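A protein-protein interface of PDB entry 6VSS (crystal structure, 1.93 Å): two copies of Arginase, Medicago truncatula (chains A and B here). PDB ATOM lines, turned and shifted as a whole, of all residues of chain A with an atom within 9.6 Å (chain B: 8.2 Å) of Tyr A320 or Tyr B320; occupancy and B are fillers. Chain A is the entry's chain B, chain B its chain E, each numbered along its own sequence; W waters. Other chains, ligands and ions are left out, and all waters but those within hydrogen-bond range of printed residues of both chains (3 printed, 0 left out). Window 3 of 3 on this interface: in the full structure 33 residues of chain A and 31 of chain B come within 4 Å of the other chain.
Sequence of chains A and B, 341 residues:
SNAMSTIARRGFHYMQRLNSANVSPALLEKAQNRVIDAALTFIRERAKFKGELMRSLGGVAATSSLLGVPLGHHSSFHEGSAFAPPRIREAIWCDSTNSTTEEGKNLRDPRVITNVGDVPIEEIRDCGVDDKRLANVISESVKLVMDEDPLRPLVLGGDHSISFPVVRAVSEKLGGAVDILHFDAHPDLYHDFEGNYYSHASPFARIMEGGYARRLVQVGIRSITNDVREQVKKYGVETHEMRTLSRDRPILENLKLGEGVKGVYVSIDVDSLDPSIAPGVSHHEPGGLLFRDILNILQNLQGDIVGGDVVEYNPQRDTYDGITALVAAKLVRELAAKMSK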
ATOM      1  N   HIS A  78     -14.312  33.185   9.163  1.00  0.00           N
ATOM      2  CA  HIS A  78     -13.354  32.083   8.898  1.00  0.00           C
ATOM      3  C   HIS A  78     -12.766  31.558  10.218  1.00  0.00           C
ATOM      4  O   HIS A  78     -12.306  32.380  11.062  1.00  0.00           O
ATOM      5  CB  HIS A  78     -12.331  32.571   7.850  1.00  0.00           C
ATOM      6  CG  HIS A  78     -11.582  31.451   7.236  1.00  0.00           C
ATOM      7  ND1 HIS A  78     -10.791  30.614   7.995  1.00  0.00           N
ATOM      8  CD2 HIS A  78     -11.534  30.985   5.955  1.00  0.00           C
ATOM      9  CE1 HIS A  78     -10.262  29.694   7.199  1.00  0.00           C
ATOM     10  NE2 HIS A  78     -10.705  29.892   5.944  1.00  0.00           N
ATOM     11  N   ARG A  87       1.608  26.555  14.883  1.00  0.00           N
ATOM     12  CA  ARG A  87       2.309  27.297  13.790  1.00  0.00           C
ATOM     13  C   ARG A  87       3.103  28.446  14.421  1.00  0.00           C
ATOM     14  O   ARG A  87       4.227  28.632  14.045  1.00  0.00           O
ATOM     15  CB  ARG A  87       1.324  27.754  12.707  1.00  0.00           C
ATOM     16  CG  ARG A  87       0.823  26.610  11.840  1.00  0.00           C
ATOM     17  CD  ARG A  87       1.917  26.078  10.931  1.00  0.00           C
ATOM     18  NE  ARG A  87       2.062  26.918   9.738  1.00  0.00           N
ATOM     19  CZ  ARG A  87       1.214  26.858   8.695  1.00  0.00           C
ATOM     20  NH1 ARG A  87       1.388  27.632   7.632  1.00  0.00           N
ATOM     21  NH2 ARG A  87       0.188  26.015   8.730  1.00  0.00           N
ATOM     22  N   GLU A  90       6.210  26.979  16.318  1.00  0.00           N
ATOM     23  CA  GLU A  90       7.260  26.574  15.367  1.00  0.00           C
ATOM     24  C   GLU A  90       7.986  27.839  14.877  1.00  0.00           C
ATOM     25  O   GLU A  90       9.182  27.791  14.686  1.00  0.00           O
ATOM     26  CB  GLU A  90       6.662  25.797  14.197  1.00  0.00           C
ATOM     27  CG  GLU A  90       7.631  25.781  13.055  1.00  0.00           C
ATOM     28  CD  GLU A  90       7.175  24.975  11.874  1.00  0.00           C
ATOM     29  OE1 GLU A  90       6.358  25.493  11.094  1.00  0.00           O
ATOM     30  OE2 GLU A  90       7.610  23.828  11.778  1.00  0.00           O
ATOM     31  N   PRO A 279      -1.110  39.191   6.133  1.00  0.00           N
ATOM     32  CA  PRO A 279      -2.165  38.670   5.296  1.00  0.00           C
ATOM     33  C   PRO A 279      -2.915  37.486   5.926  1.00  0.00           C
ATOM     34  O   PRO A 279      -4.033  37.284   5.624  1.00  0.00           O
ATOM     35  CB  PRO A 279      -1.465  38.280   3.989  1.00  0.00           C
ATOM     36  CG  PRO A 279      -0.021  38.175   4.329  1.00  0.00           C
ATOM     37  CD  PRO A 279       0.205  39.018   5.559  1.00  0.00           C
ATOM     38  N   GLY A 280      -2.253  36.779   6.828  1.00  0.00           N
ATOM     39  CA  GLY A 280      -2.785  35.575   7.469  1.00  0.00           C
ATOM     40  C   GLY A 280      -3.776  35.926   8.555  1.00  0.00           C
ATOM     41  O   GLY A 280      -3.460  35.675   9.688  1.00  0.00           O
ATOM     42  N   TYR A 313      -4.301  35.111  14.296  1.00  0.00           N
ATOM     43  CA  TYR A 313      -3.450  34.532  13.224  1.00  0.00           C
ATOM     44  C   TYR A 313      -4.258  33.363  12.607  1.00  0.00           C
ATOM     45  O   TYR A 313      -4.715  32.495  13.353  1.00  0.00           O
ATOM     46  CB  TYR A 313      -2.063  34.054  13.671  1.00  0.00           C
ATOM     47  CG  TYR A 313      -1.339  33.281  12.599  1.00  0.00           C
ATOM     48  CD1 TYR A 313      -1.308  33.729  11.288  1.00  0.00           C
ATOM     49  CD2 TYR A 313      -0.673  32.090  12.872  1.00  0.00           C
ATOM     50  CE1 TYR A 313      -0.630  33.027  10.295  1.00  0.00           C
ATOM     51  CE2 TYR A 313      -0.039  31.353  11.879  1.00  0.00           C
ATOM     52  CZ  TYR A 313       0.016  31.839  10.591  1.00  0.00           C
ATOM     53  OH  TYR A 313       0.708  31.151   9.608  1.00  0.00           O
ATOM     54  N   ASN A 314      -4.414  33.366  11.274  1.00  0.00           N
ATOM     55  CA  ASN A 314      -5.136  32.330  10.493  1.00  0.00           C
ATOM     56  C   ASN A 314      -4.154  31.761   9.481  1.00  0.00           C
ATOM     57  O   ASN A 314      -3.979  32.288   8.382  1.00  0.00           O
ATOM     58  CB  ASN A 314      -6.373  32.982   9.852  1.00  0.00           C
ATOM     59  CG  ASN A 314      -7.265  31.969   9.162  1.00  0.00           C
ATOM     60  OD1 ASN A 314      -6.795  30.881   8.831  1.00  0.00           O
ATOM     61  ND2 ASN A 314      -8.538  32.321   8.958  1.00  0.00           N
ATOM     62  N   PRO A 315      -3.521  30.617   9.772  1.00  0.00           N
ATOM     63  CA  PRO A 315      -2.572  30.022   8.844  1.00  0.00           C
ATOM     64  C   PRO A 315      -3.177  29.561   7.510  1.00  0.00           C
ATOM     65  O   PRO A 315      -2.485  29.510   6.547  1.00  0.00           O
ATOM     66  CB  PRO A 315      -1.999  28.808   9.598  1.00  0.00           C
ATOM     67  CG  PRO A 315      -2.800  28.645  10.845  1.00  0.00           C
ATOM     68  CD  PRO A 315      -3.679  29.857  11.014  1.00  0.00           C
ATOM     69  N   GLN A 316      -4.473  29.300   7.460  1.00  0.00           N
ATOM     70  CA  GLN A 316      -5.183  28.982   6.190  1.00  0.00           C
ATOM     71  C   GLN A 316      -5.246  30.207   5.294  1.00  0.00           C
ATOM     72  O   GLN A 316      -5.592  29.990   4.188  1.00  0.00           O
ATOM     73  CB  GLN A 316      -6.637  28.558   6.389  1.00  0.00           C
ATOM     74  CG  GLN A 316      -6.731  27.219   7.081  1.00  0.00           C
ATOM     75  CD  GLN A 316      -8.121  26.649   7.211  1.00  0.00           C
ATOM     76  OE1 GLN A 316      -8.819  26.937   8.167  1.00  0.00           O
ATOM     77  NE2 GLN A 316      -8.482  25.732   6.320  1.00  0.00           N
ATOM     78  N   ARG A 317      -5.010  31.413   5.783  1.00  0.00           N
ATOM     79  CA  ARG A 317      -5.086  32.590   4.885  1.00  0.00           C
ATOM     80  C   ARG A 317      -3.708  33.236   4.742  1.00  0.00           C
ATOM     81  O   ARG A 317      -3.630  34.309   4.177  1.00  0.00           O
ATOM     82  CB  ARG A 317      -6.162  33.559   5.362  1.00  0.00           C
ATOM     83  CG  ARG A 317      -7.500  32.876   5.581  1.00  0.00           C
ATOM     84  CD  ARG A 317      -8.732  33.568   5.085  1.00  0.00           C
ATOM     85  NE  ARG A 317      -8.604  34.983   5.270  1.00  0.00           N
ATOM     86  CZ  ARG A 317      -8.996  35.884   4.400  1.00  0.00           C
ATOM     87  NH1 ARG A 317      -9.575  35.522   3.272  1.00  0.00           N
ATOM     88  NH2 ARG A 317      -8.828  37.154   4.672  1.00  0.00           N
ATOM     89  N   ASP A 318      -2.671  32.555   5.220  1.00  0.00           N
ATOM     90  CA  ASP A 318      -1.283  33.074   5.182  1.00  0.00           C
ATOM     91  C   ASP A 318      -0.688  32.877   3.780  1.00  0.00           C
ATOM     92  O   ASP A 318      -1.260  32.168   2.973  1.00  0.00           O
ATOM     93  CB  ASP A 318      -0.430  32.397   6.254  1.00  0.00           C
ATOM     94  CG  ASP A 318       0.771  33.191   6.742  1.00  0.00           C
ATOM     95  OD1 ASP A 318       1.088  34.192   6.126  1.00  0.00           O
ATOM     96  OD2 ASP A 318       1.376  32.775   7.685  1.00  0.00           O
ATOM     97  N   THR A 319       0.480  33.452   3.529  1.00  0.00           N
ATOM     98  CA  THR A 319       1.159  33.215   2.237  1.00  0.00           C
ATOM     99  C   THR A 319       1.866  31.853   2.288  1.00  0.00           C
ATOM    100  O   THR A 319       2.014  31.262   3.356  1.00  0.00           O
ATOM    101  CB  THR A 319       2.125  34.336   1.859  1.00  0.00           C
ATOM    102  OG1 THR A 319       2.975  34.499   2.978  1.00  0.00           O
ATOM    103  CG2 THR A 319       1.462  35.662   1.591  1.00  0.00           C
ATOM    104  N   TYR A 320       2.400  31.415   1.159  1.00  0.00           N
ATOM    105  CA  TYR A 320       3.059  30.089   1.132  1.00  0.00           C
ATOM    106  C   TYR A 320       4.283  30.047   2.056  1.00  0.00           C
ATOM    107  O   TYR A 320       4.507  29.019   2.631  1.00  0.00           O
ATOM    108  CB  TYR A 320       3.252  29.632  -0.311  1.00  0.00           C
ATOM    109  CG  TYR A 320       3.728  28.219  -0.493  1.00  0.00           C
ATOM    110  CD1 TYR A 320       4.928  27.810   0.021  1.00  0.00           C
ATOM    111  CD2 TYR A 320       2.957  27.264  -1.119  1.00  0.00           C
ATOM    112  CE1 TYR A 320       5.443  26.551  -0.229  1.00  0.00           C
ATOM    113  CE2 TYR A 320       3.428  25.981  -1.331  1.00  0.00           C
ATOM    114  CZ  TYR A 320       4.676  25.614  -0.880  1.00  0.00           C
ATOM    115  OH  TYR A 320       5.154  24.361  -1.081  1.00  0.00           O
ATOM    116  N   ASP A 321       5.004  31.157   2.213  1.00  0.00           N
ATOM    117  CA  ASP A 321       6.211  31.267   3.076  1.00  0.00           C
ATOM    118  C   ASP A 321       5.850  31.385   4.567  1.00  0.00           C
ATOM    119  O   ASP A 321       6.739  31.383   5.343  1.00  0.00           O
ATOM    120  CB  ASP A 321       7.080  32.445   2.641  1.00  0.00           C
ATOM    121  CG  ASP A 321       6.332  33.765   2.546  1.00  0.00           C
ATOM    122  OD1 ASP A 321       5.402  33.972   3.306  1.00  0.00           O
ATOM    123  OD2 ASP A 321       6.725  34.595   1.760  1.00  0.00           O
ATOM    124  N   GLY A 322       4.581  31.496   4.932  1.00  0.00           N
ATOM    125  CA  GLY A 322       4.196  31.600   6.351  1.00  0.00           C
ATOM    126  C   GLY A 322       4.631  32.913   6.975  1.00  0.00           C
ATOM    127  O   GLY A 322       4.933  32.908   8.142  1.00  0.00           O
ATOM    128  N   ILE A 323       4.640  34.003   6.211  1.00  0.00           N
ATOM    129  CA  ILE A 323       5.079  35.317   6.768  1.00  0.00           C
ATOM    130  C   ILE A 323       4.274  35.681   8.029  1.00  0.00           C
ATOM    131  O   ILE A 323       4.867  36.101   8.981  1.00  0.00           O
ATOM    132  CB  ILE A 323       5.072  36.429   5.696  1.00  0.00           C
ATOM    133  CG1 ILE A 323       5.803  37.687   6.157  1.00  0.00           C
ATOM    134  CG2 ILE A 323       3.691  36.746   5.169  1.00  0.00           C
ATOM    135  CD1 ILE A 323       7.128  37.431   6.806  1.00  0.00           C
ATOM    136  N   THR A 324       2.979  35.463   8.036  1.00  0.00           N
ATOM    137  CA  THR A 324       2.180  35.880   9.209  1.00  0.00           C
ATOM    138  C   THR A 324       2.519  35.022  10.417  1.00  0.00           C
ATOM    139  O   THR A 324       2.432  35.532  11.505  1.00  0.00           O
ATOM    140  CB  THR A 324       0.684  35.940   8.952  1.00  0.00           C
ATOM    141  OG1 THR A 324       0.570  36.602   7.716  1.00  0.00           O
ATOM    142  CG2 THR A 324      -0.102  36.697   9.990  1.00  0.00           C
ATOM    143  N   ALA A 325       2.909  33.768  10.261  1.00  0.00           N
ATOM    144  CA  ALA A 325       3.353  32.953  11.415  1.00  0.00           C
ATOM    145  C   ALA A 325       4.538  33.659  12.103  1.00  0.00           C
ATOM    146  O   ALA A 325       4.569  33.774  13.350  1.00  0.00           O
ATOM    147  CB  ALA A 325       3.707  31.554  10.976  1.00  0.00           C
ATOM    148  N   PHE B  77      13.267  16.126   5.212  1.00  0.00           N
ATOM    149  CA  PHE B  77      13.245  17.325   4.341  1.00  0.00           C
ATOM    150  C   PHE B  77      12.407  18.466   4.953  1.00  0.00           C
ATOM    151  O   PHE B  77      12.969  19.550   5.035  1.00  0.00           O
ATOM    152  CB  PHE B  77      12.802  16.956   2.921  1.00  0.00           C
ATOM    153  CG  PHE B  77      12.730  18.123   1.981  1.00  0.00           C
ATOM    154  CD1 PHE B  77      13.884  18.703   1.485  1.00  0.00           C
ATOM    155  CD2 PHE B  77      11.502  18.650   1.599  1.00  0.00           C
ATOM    156  CE1 PHE B  77      13.815  19.799   0.632  1.00  0.00           C
ATOM    157  CE2 PHE B  77      11.431  19.746   0.748  1.00  0.00           C
ATOM    158  CZ  PHE B  77      12.589  20.332   0.281  1.00  0.00           C
ATOM    159  N   HIS B  78      11.173  18.218   5.389  1.00  0.00           N
ATOM    160  CA  HIS B  78      10.250  19.220   5.951  1.00  0.00           C
ATOM    161  C   HIS B  78       9.389  18.494   7.006  1.00  0.00           C
ATOM    162  O   HIS B  78       9.019  17.310   6.750  1.00  0.00           O
ATOM    163  CB  HIS B  78       9.515  19.849   4.750  1.00  0.00           C
ATOM    164  CG  HIS B  78       8.812  21.147   5.014  1.00  0.00           C
ATOM    165  ND1 HIS B  78       7.667  21.251   5.845  1.00  0.00           N
ATOM    166  CD2 HIS B  78       9.109  22.395   4.622  1.00  0.00           C
ATOM    167  CE1 HIS B  78       7.304  22.527   5.916  1.00  0.00           C
ATOM    168  NE2 HIS B  78       8.164  23.226   5.153  1.00  0.00           N
ATOM    169  N   ARG B  87      -6.143  19.406  10.345  1.00  0.00           N
ATOM    170  CA  ARG B  87      -6.501  19.872   8.990  1.00  0.00           C
ATOM    171  C   ARG B  87      -7.299  18.788   8.271  1.00  0.00           C
ATOM    172  O   ARG B  87      -8.273  19.129   7.578  1.00  0.00           O
ATOM    173  CB  ARG B  87      -5.261  20.261   8.182  1.00  0.00           C
ATOM    174  CG  ARG B  87      -5.104  21.767   8.095  1.00  0.00           C
ATOM    175  CD  ARG B  87      -6.294  22.424   7.371  1.00  0.00           C
ATOM    176  NE  ARG B  87      -5.854  22.933   6.087  1.00  0.00           N
ATOM    177  CZ  ARG B  87      -4.764  23.706   5.933  1.00  0.00           C
ATOM    178  NH1 ARG B  87      -4.038  24.044   6.989  1.00  0.00           N
ATOM    179  NH2 ARG B  87      -4.412  24.130   4.738  1.00  0.00           N
ATOM    180  N   PRO B 279      -0.041  18.062  -4.063  1.00  0.00           N
ATOM    181  CA  PRO B 279       1.135  18.907  -3.868  1.00  0.00           C
ATOM    182  C   PRO B 279       1.465  19.103  -2.373  1.00  0.00           C
ATOM    183  O   PRO B 279       2.593  19.387  -2.068  1.00  0.00           O
ATOM    184  CB  PRO B 279       0.703  20.219  -4.548  1.00  0.00           C
ATOM    185  CG  PRO B 279      -0.792  20.262  -4.310  1.00  0.00           C
ATOM    186  CD  PRO B 279      -1.202  18.820  -4.552  1.00  0.00           C
ATOM    187  N   GLY B 280       0.519  18.866  -1.466  1.00  0.00           N
ATOM    188  CA  GLY B 280       0.715  19.048  -0.002  1.00  0.00           C
ATOM    189  C   GLY B 280       1.425  17.879   0.643  1.00  0.00           C
ATOM    190  O   GLY B 280       0.780  17.216   1.469  1.00  0.00           O
ATOM    191  N   VAL B 281       2.676  17.606   0.259  1.00  0.00           N
ATOM    192  CA  VAL B 281       3.552  16.559   0.891  1.00  0.00           C
ATOM    193  C   VAL B 281       4.995  17.086   0.935  1.00  0.00           C
ATOM    194  O   VAL B 281       5.276  18.007   0.188  1.00  0.00           O
ATOM    195  CB  VAL B 281       3.531  15.236   0.108  1.00  0.00           C
ATOM    196  CG1 VAL B 281       2.140  14.703   0.012  1.00  0.00           C
ATOM    197  CG2 VAL B 281       4.116  15.411  -1.293  1.00  0.00           C
ATOM    198  N   HIS B 284       7.884  15.491  -3.305  1.00  0.00           N
ATOM    199  CA  HIS B 284       7.312  15.471  -4.666  1.00  0.00           C
ATOM    200  C   HIS B 284       8.086  14.438  -5.504  1.00  0.00           C
ATOM    201  O   HIS B 284       9.298  14.528  -5.573  1.00  0.00           O
ATOM    202  CB  HIS B 284       7.340  16.859  -5.223  1.00  0.00           C
ATOM    203  CG  HIS B 284       6.392  17.772  -4.556  1.00  0.00           C
ATOM    204  ND1 HIS B 284       6.492  19.105  -4.690  1.00  0.00           N
ATOM    205  CD2 HIS B 284       5.323  17.552  -3.777  1.00  0.00           C
ATOM    206  CE1 HIS B 284       5.532  19.684  -4.003  1.00  0.00           C
ATOM    207  NE2 HIS B 284       4.820  18.778  -3.420  1.00  0.00           N
ATOM    208  N   ASN B 314       1.277  17.284   4.339  1.00  0.00           N
ATOM    209  CA  ASN B 314       2.032  18.484   4.778  1.00  0.00           C
ATOM    210  C   ASN B 314       1.195  19.721   4.474  1.00  0.00           C
ATOM    211  O   ASN B 314       1.277  20.235   3.338  1.00  0.00           O
ATOM    212  CB  ASN B 314       3.373  18.545   4.046  1.00  0.00           C
ATOM    213  CG  ASN B 314       4.316  19.531   4.697  1.00  0.00           C
ATOM    214  OD1 ASN B 314       3.831  20.583   5.147  1.00  0.00           O
ATOM    215  ND2 ASN B 314       5.611  19.203   4.833  1.00  0.00           N
ATOM    216  N   PRO B 315       0.388  20.275   5.433  1.00  0.00           N
ATOM    217  CA  PRO B 315      -0.393  21.490   5.160  1.00  0.00           C
ATOM    218  C   PRO B 315       0.436  22.696   4.724  1.00  0.00           C
ATOM    219  O   PRO B 315      -0.070  23.484   3.962  1.00  0.00           O
ATOM    220  CB  PRO B 315      -1.157  21.852   6.460  1.00  0.00           C
ATOM    221  CG  PRO B 315      -0.561  20.901   7.486  1.00  0.00           C
ATOM    222  CD  PRO B 315       0.080  19.742   6.758  1.00  0.00           C
ATOM    223  N   GLN B 316       1.666  22.799   5.202  1.00  0.00           N
ATOM    224  CA  GLN B 316       2.535  23.937   4.844  1.00  0.00           C
ATOM    225  C   GLN B 316       2.974  23.884   3.378  1.00  0.00           C
ATOM    226  O   GLN B 316       3.531  24.861   2.967  1.00  0.00           O
ATOM    227  CB  GLN B 316       3.753  24.001   5.755  1.00  0.00           C
ATOM    228  CG  GLN B 316       3.390  24.316   7.190  1.00  0.00           C
ATOM    229  CD  GLN B 316       4.561  24.290   8.131  1.00  0.00           C
ATOM    230  OE1 GLN B 316       5.302  23.339   8.197  1.00  0.00           O
ATOM    231  NE2 GLN B 316       4.706  25.352   8.893  1.00  0.00           N
ATOM    232  N   ARG B 317       2.721  22.807   2.640  1.00  0.00           N
ATOM    233  CA  ARG B 317       3.157  22.742   1.219  1.00  0.00           C
ATOM    234  C   ARG B 317       1.945  22.549   0.310  1.00  0.00           C
ATOM    235  O   ARG B 317       2.101  22.351  -0.869  1.00  0.00           O
ATOM    236  CB  ARG B 317       4.240  21.689   0.991  1.00  0.00           C
ATOM    237  CG  ARG B 317       5.309  21.654   2.065  1.00  0.00           C
ATOM    238  CD  ARG B 317       6.730  21.464   1.600  1.00  0.00           C
ATOM    239  NE  ARG B 317       6.903  20.428   0.621  1.00  0.00           N
ATOM    240  CZ  ARG B 317       7.641  20.574  -0.461  1.00  0.00           C
ATOM    241  NH1 ARG B 317       8.283  21.700  -0.677  1.00  0.00           N
ATOM    242  NH2 ARG B 317       7.750  19.591  -1.313  1.00  0.00           N
ATOM    243  N   ASP B 318       0.762  22.646   0.889  1.00  0.00           N
ATOM    244  CA  ASP B 318      -0.482  22.519   0.118  1.00  0.00           C
ATOM    245  C   ASP B 318      -0.719  23.846  -0.635  1.00  0.00           C
ATOM    246  O   ASP B 318      -0.156  24.881  -0.286  1.00  0.00           O
ATOM    247  CB  ASP B 318      -1.578  22.072   1.083  1.00  0.00           C
ATOM    248  CG  ASP B 318      -2.781  21.387   0.458  1.00  0.00           C
ATOM    249  OD1 ASP B 318      -2.807  21.255  -0.746  1.00  0.00           O
ATOM    250  OD2 ASP B 318      -3.679  21.018   1.199  1.00  0.00           O
ATOM    251  N   THR B 319      -1.652  23.838  -1.590  1.00  0.00           N
ATOM    252  CA  THR B 319      -2.097  25.036  -2.324  1.00  0.00           C
ATOM    253  C   THR B 319      -3.001  25.840  -1.403  1.00  0.00           C
ATOM    254  O   THR B 319      -3.489  25.299  -0.413  1.00  0.00           O
ATOM    255  CB  THR B 319      -2.842  24.654  -3.613  1.00  0.00           C
ATOM    256  OG1 THR B 319      -3.964  23.893  -3.153  1.00  0.00           O
ATOM    257  CG2 THR B 319      -1.989  23.909  -4.621  1.00  0.00           C
ATOM    258  N   TYR B 320      -3.260  27.088  -1.757  1.00  0.00           N
ATOM    259  CA  TYR B 320      -4.102  27.963  -0.916  1.00  0.00           C
ATOM    260  C   TYR B 320      -5.491  27.349  -0.725  1.00  0.00           C
ATOM    261  O   TYR B 320      -6.055  27.560   0.314  1.00  0.00           O
ATOM    262  CB  TYR B 320      -4.113  29.389  -1.467  1.00  0.00           C
ATOM    263  CG  TYR B 320      -2.808  30.142  -1.371  1.00  0.00           C
ATOM    264  CD1 TYR B 320      -2.072  30.187  -0.202  1.00  0.00           C
ATOM    265  CD2 TYR B 320      -2.304  30.821  -2.459  1.00  0.00           C
ATOM    266  CE1 TYR B 320      -0.859  30.847  -0.134  1.00  0.00           C
ATOM    267  CE2 TYR B 320      -1.112  31.515  -2.402  1.00  0.00           C
ATOM    268  CZ  TYR B 320      -0.383  31.537  -1.233  1.00  0.00           C
ATOM    269  OH  TYR B 320       0.786  32.234  -1.171  1.00  0.00           O
ATOM    270  N   ASP B 321      -5.984  26.564  -1.682  1.00  0.00           N
ATOM    271  CA  ASP B 321      -7.356  26.007  -1.579  1.00  0.00           C
ATOM    272  C   ASP B 321      -7.372  24.786  -0.655  1.00  0.00           C
ATOM    273  O   ASP B 321      -8.459  24.272  -0.464  1.00  0.00           O
ATOM    274  CB  ASP B 321      -7.935  25.656  -2.970  1.00  0.00           C
ATOM    275  CG  ASP B 321      -7.030  24.764  -3.798  1.00  0.00           C
ATOM    276  OD1 ASP B 321      -6.227  24.021  -3.203  1.00  0.00           O
ATOM    277  OD2 ASP B 321      -7.080  24.849  -5.021  1.00  0.00           O
ATOM    278  N   GLY B 322      -6.227  24.285  -0.157  1.00  0.00           N
ATOM    279  CA  GLY B 322      -6.180  23.039   0.636  1.00  0.00           C
ATOM    280  C   GLY B 322      -6.676  21.800  -0.128  1.00  0.00           C
ATOM    281  O   GLY B 322      -7.406  21.009   0.448  1.00  0.00           O
ATOM    282  N   ILE B 323      -6.303  21.612  -1.401  1.00  0.00           N
ATOM    283  CA  ILE B 323      -6.761  20.443  -2.214  1.00  0.00           C
ATOM    284  C   ILE B 323      -6.237  19.152  -1.551  1.00  0.00           C
ATOM    285  O   ILE B 323      -6.999  18.162  -1.362  1.00  0.00           O
ATOM    286  CB  ILE B 323      -6.263  20.586  -3.681  1.00  0.00           C
ATOM    287  CG1 ILE B 323      -6.856  19.507  -4.580  1.00  0.00           C
ATOM    288  CG2 ILE B 323      -4.748  20.559  -3.794  1.00  0.00           C
ATOM    289  CD1 ILE B 323      -8.306  19.308  -4.303  1.00  0.00           C
ATOM    290  N   THR B 324      -4.980  19.165  -1.114  1.00  0.00           N
ATOM    291  CA  THR B 324      -4.351  17.966  -0.524  1.00  0.00           C
ATOM    292  C   THR B 324      -5.038  17.542   0.793  1.00  0.00           C
ATOM    293  O   THR B 324      -5.139  16.351   1.011  1.00  0.00           O
ATOM    294  CB  THR B 324      -2.836  18.052  -0.436  1.00  0.00           C
ATOM    295  OG1 THR B 324      -2.267  18.668  -1.604  1.00  0.00           O
ATOM    296  CG2 THR B 324      -2.305  16.637  -0.256  1.00  0.00           C
HETATM  297  O   HOH W   1       7.472  22.609   9.514  1.00  0.00           O
HETATM  298  O   HOH W   2      -1.929  24.419   9.637  1.00  0.00           O
HETATM  299  O   HOH W   3       4.086  22.360  -2.523  1.00  0.00           O
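Gln A316 touches Arg B87 (NE2 to NE, 3.8 Å). Tyr B320 touches Asp A318 (CE1 to O, 3.4 Å). Thr A319 touches Tyr B320 (CA to OH, 3.6 Å). Tyr A320 touches Arg B317. Asp B318 touches Tyr A320.
The side-chain carboxylate of Asp A318 sits at hydrogen-bond distance from the side-chain hydroxyl of Tyr A313, 2.6 Å away. OD1 of Asp A318 sits at hydrogen-bond distance from OG1 of Thr A324, at 2.9 Å. The side-chain hydroxyl (OG1) of Thr A319 sits at hydrogen-bond distance from the side-chain carboxylate (OD1) of Asp A321. The backbone carbonyl oxygen of Val B281 lies within hydrogen-bond range of the guanidinium group of Arg B317, at 2.9 Å. The side-chain amide oxygen (OD1) of Asn B314 sits at hydrogen-bond distance from the backbone NH (N) of Gln B316 (3.1 Å). The side-chain carboxylate (OD1) of Asp B318 sits at hydrogen-bond distance from the side-chain hydroxyl (OG1) of Thr B324 (2.8 Å).
Hydrophobic or aromatic side chains of chain B within 4 Å of the printed part of chain A: Tyr B320. Hydrophobic or aromatic side chains of chain A within 4 Å of the printed part of chain B: Tyr A320. Among the printed residues, no Asp or Glu carboxylate lies within 4 Å of a Lys or Arg side-chain nitrogen of the other chain.
Of the printed residues of chain B, Glu A90 touches Gln B316. Of the printed residues of chain B, Gln A316 touches Arg B87 (3.8 Å). Of the printed residues of chain B, Asp A318 touches Tyr B320. Printed residues of chain B within 4 Å of Thr A319: Tyr B320 (3.6 Å). Tyr A320 touches three residues of chain B. Asp A321 touches none of the printed residues of chain B. Arg B317 touches one residue of chain A. Of the printed residues of chain A, Asp B318 touches Tyr A320. No residue of chain A comes within 4 Å of Thr B319. The nearest residue of chain B that does not touch Tyr A320 is Gln B316 (4.1 Å). The nearest residue of chain A that does not touch Tyr B320 is Gln A316 (4.6 Å).
Arg A87 touches Gln B316, and with the chains exchanged Gln A316 touches Arg B87. Asp A318 touches Tyr B320, and with the chains exchanged Tyr A320 touches Asp B318. Tyr A320 touches Arg B317, but with the chains exchanged Arg A317 does not touch Tyr B320 (6.0 Å). Tyr A320 touches its own counterpart, Tyr B320. Positions printed for both chains: 78, 87, 279, 280, 314, 315, 316, 317, 318, 319, 320, 321, 322, 323 and 324. Of the 8 pairs that touch across the chains among the printed residues, 5 have their exchanged pair printed and touching as well.
Water W1 lies within hydrogen-bond range of the side-chain carboxylate (OE2) of Glu A90 (2.6 Å) and the side-chain amide oxygen (OE1) of Gln B316 (2.6 Å). Water W3 lies within hydrogen-bond range of O of Arg B317, OH of Tyr A320 and O of Pro B279. Water W2 lies within hydrogen-bond range of NH2 of Arg A87 (2.8 Å) and NH1 of Arg B87 (3.4 Å).
The guanidinium group (NE) of Arg A87 lies close to the side-chain amide nitrogen (NE2) of Gln B316. The side-chain amide nitrogen (NE2) of Gln B316 sits at hydrogen-bond distance from the side-chain carboxylate (OE1) of Glu A90, 2.8 Å away. N of Tyr A320 is in hydrogen-bond range of OH of Tyr B320, 3.0 Å away.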
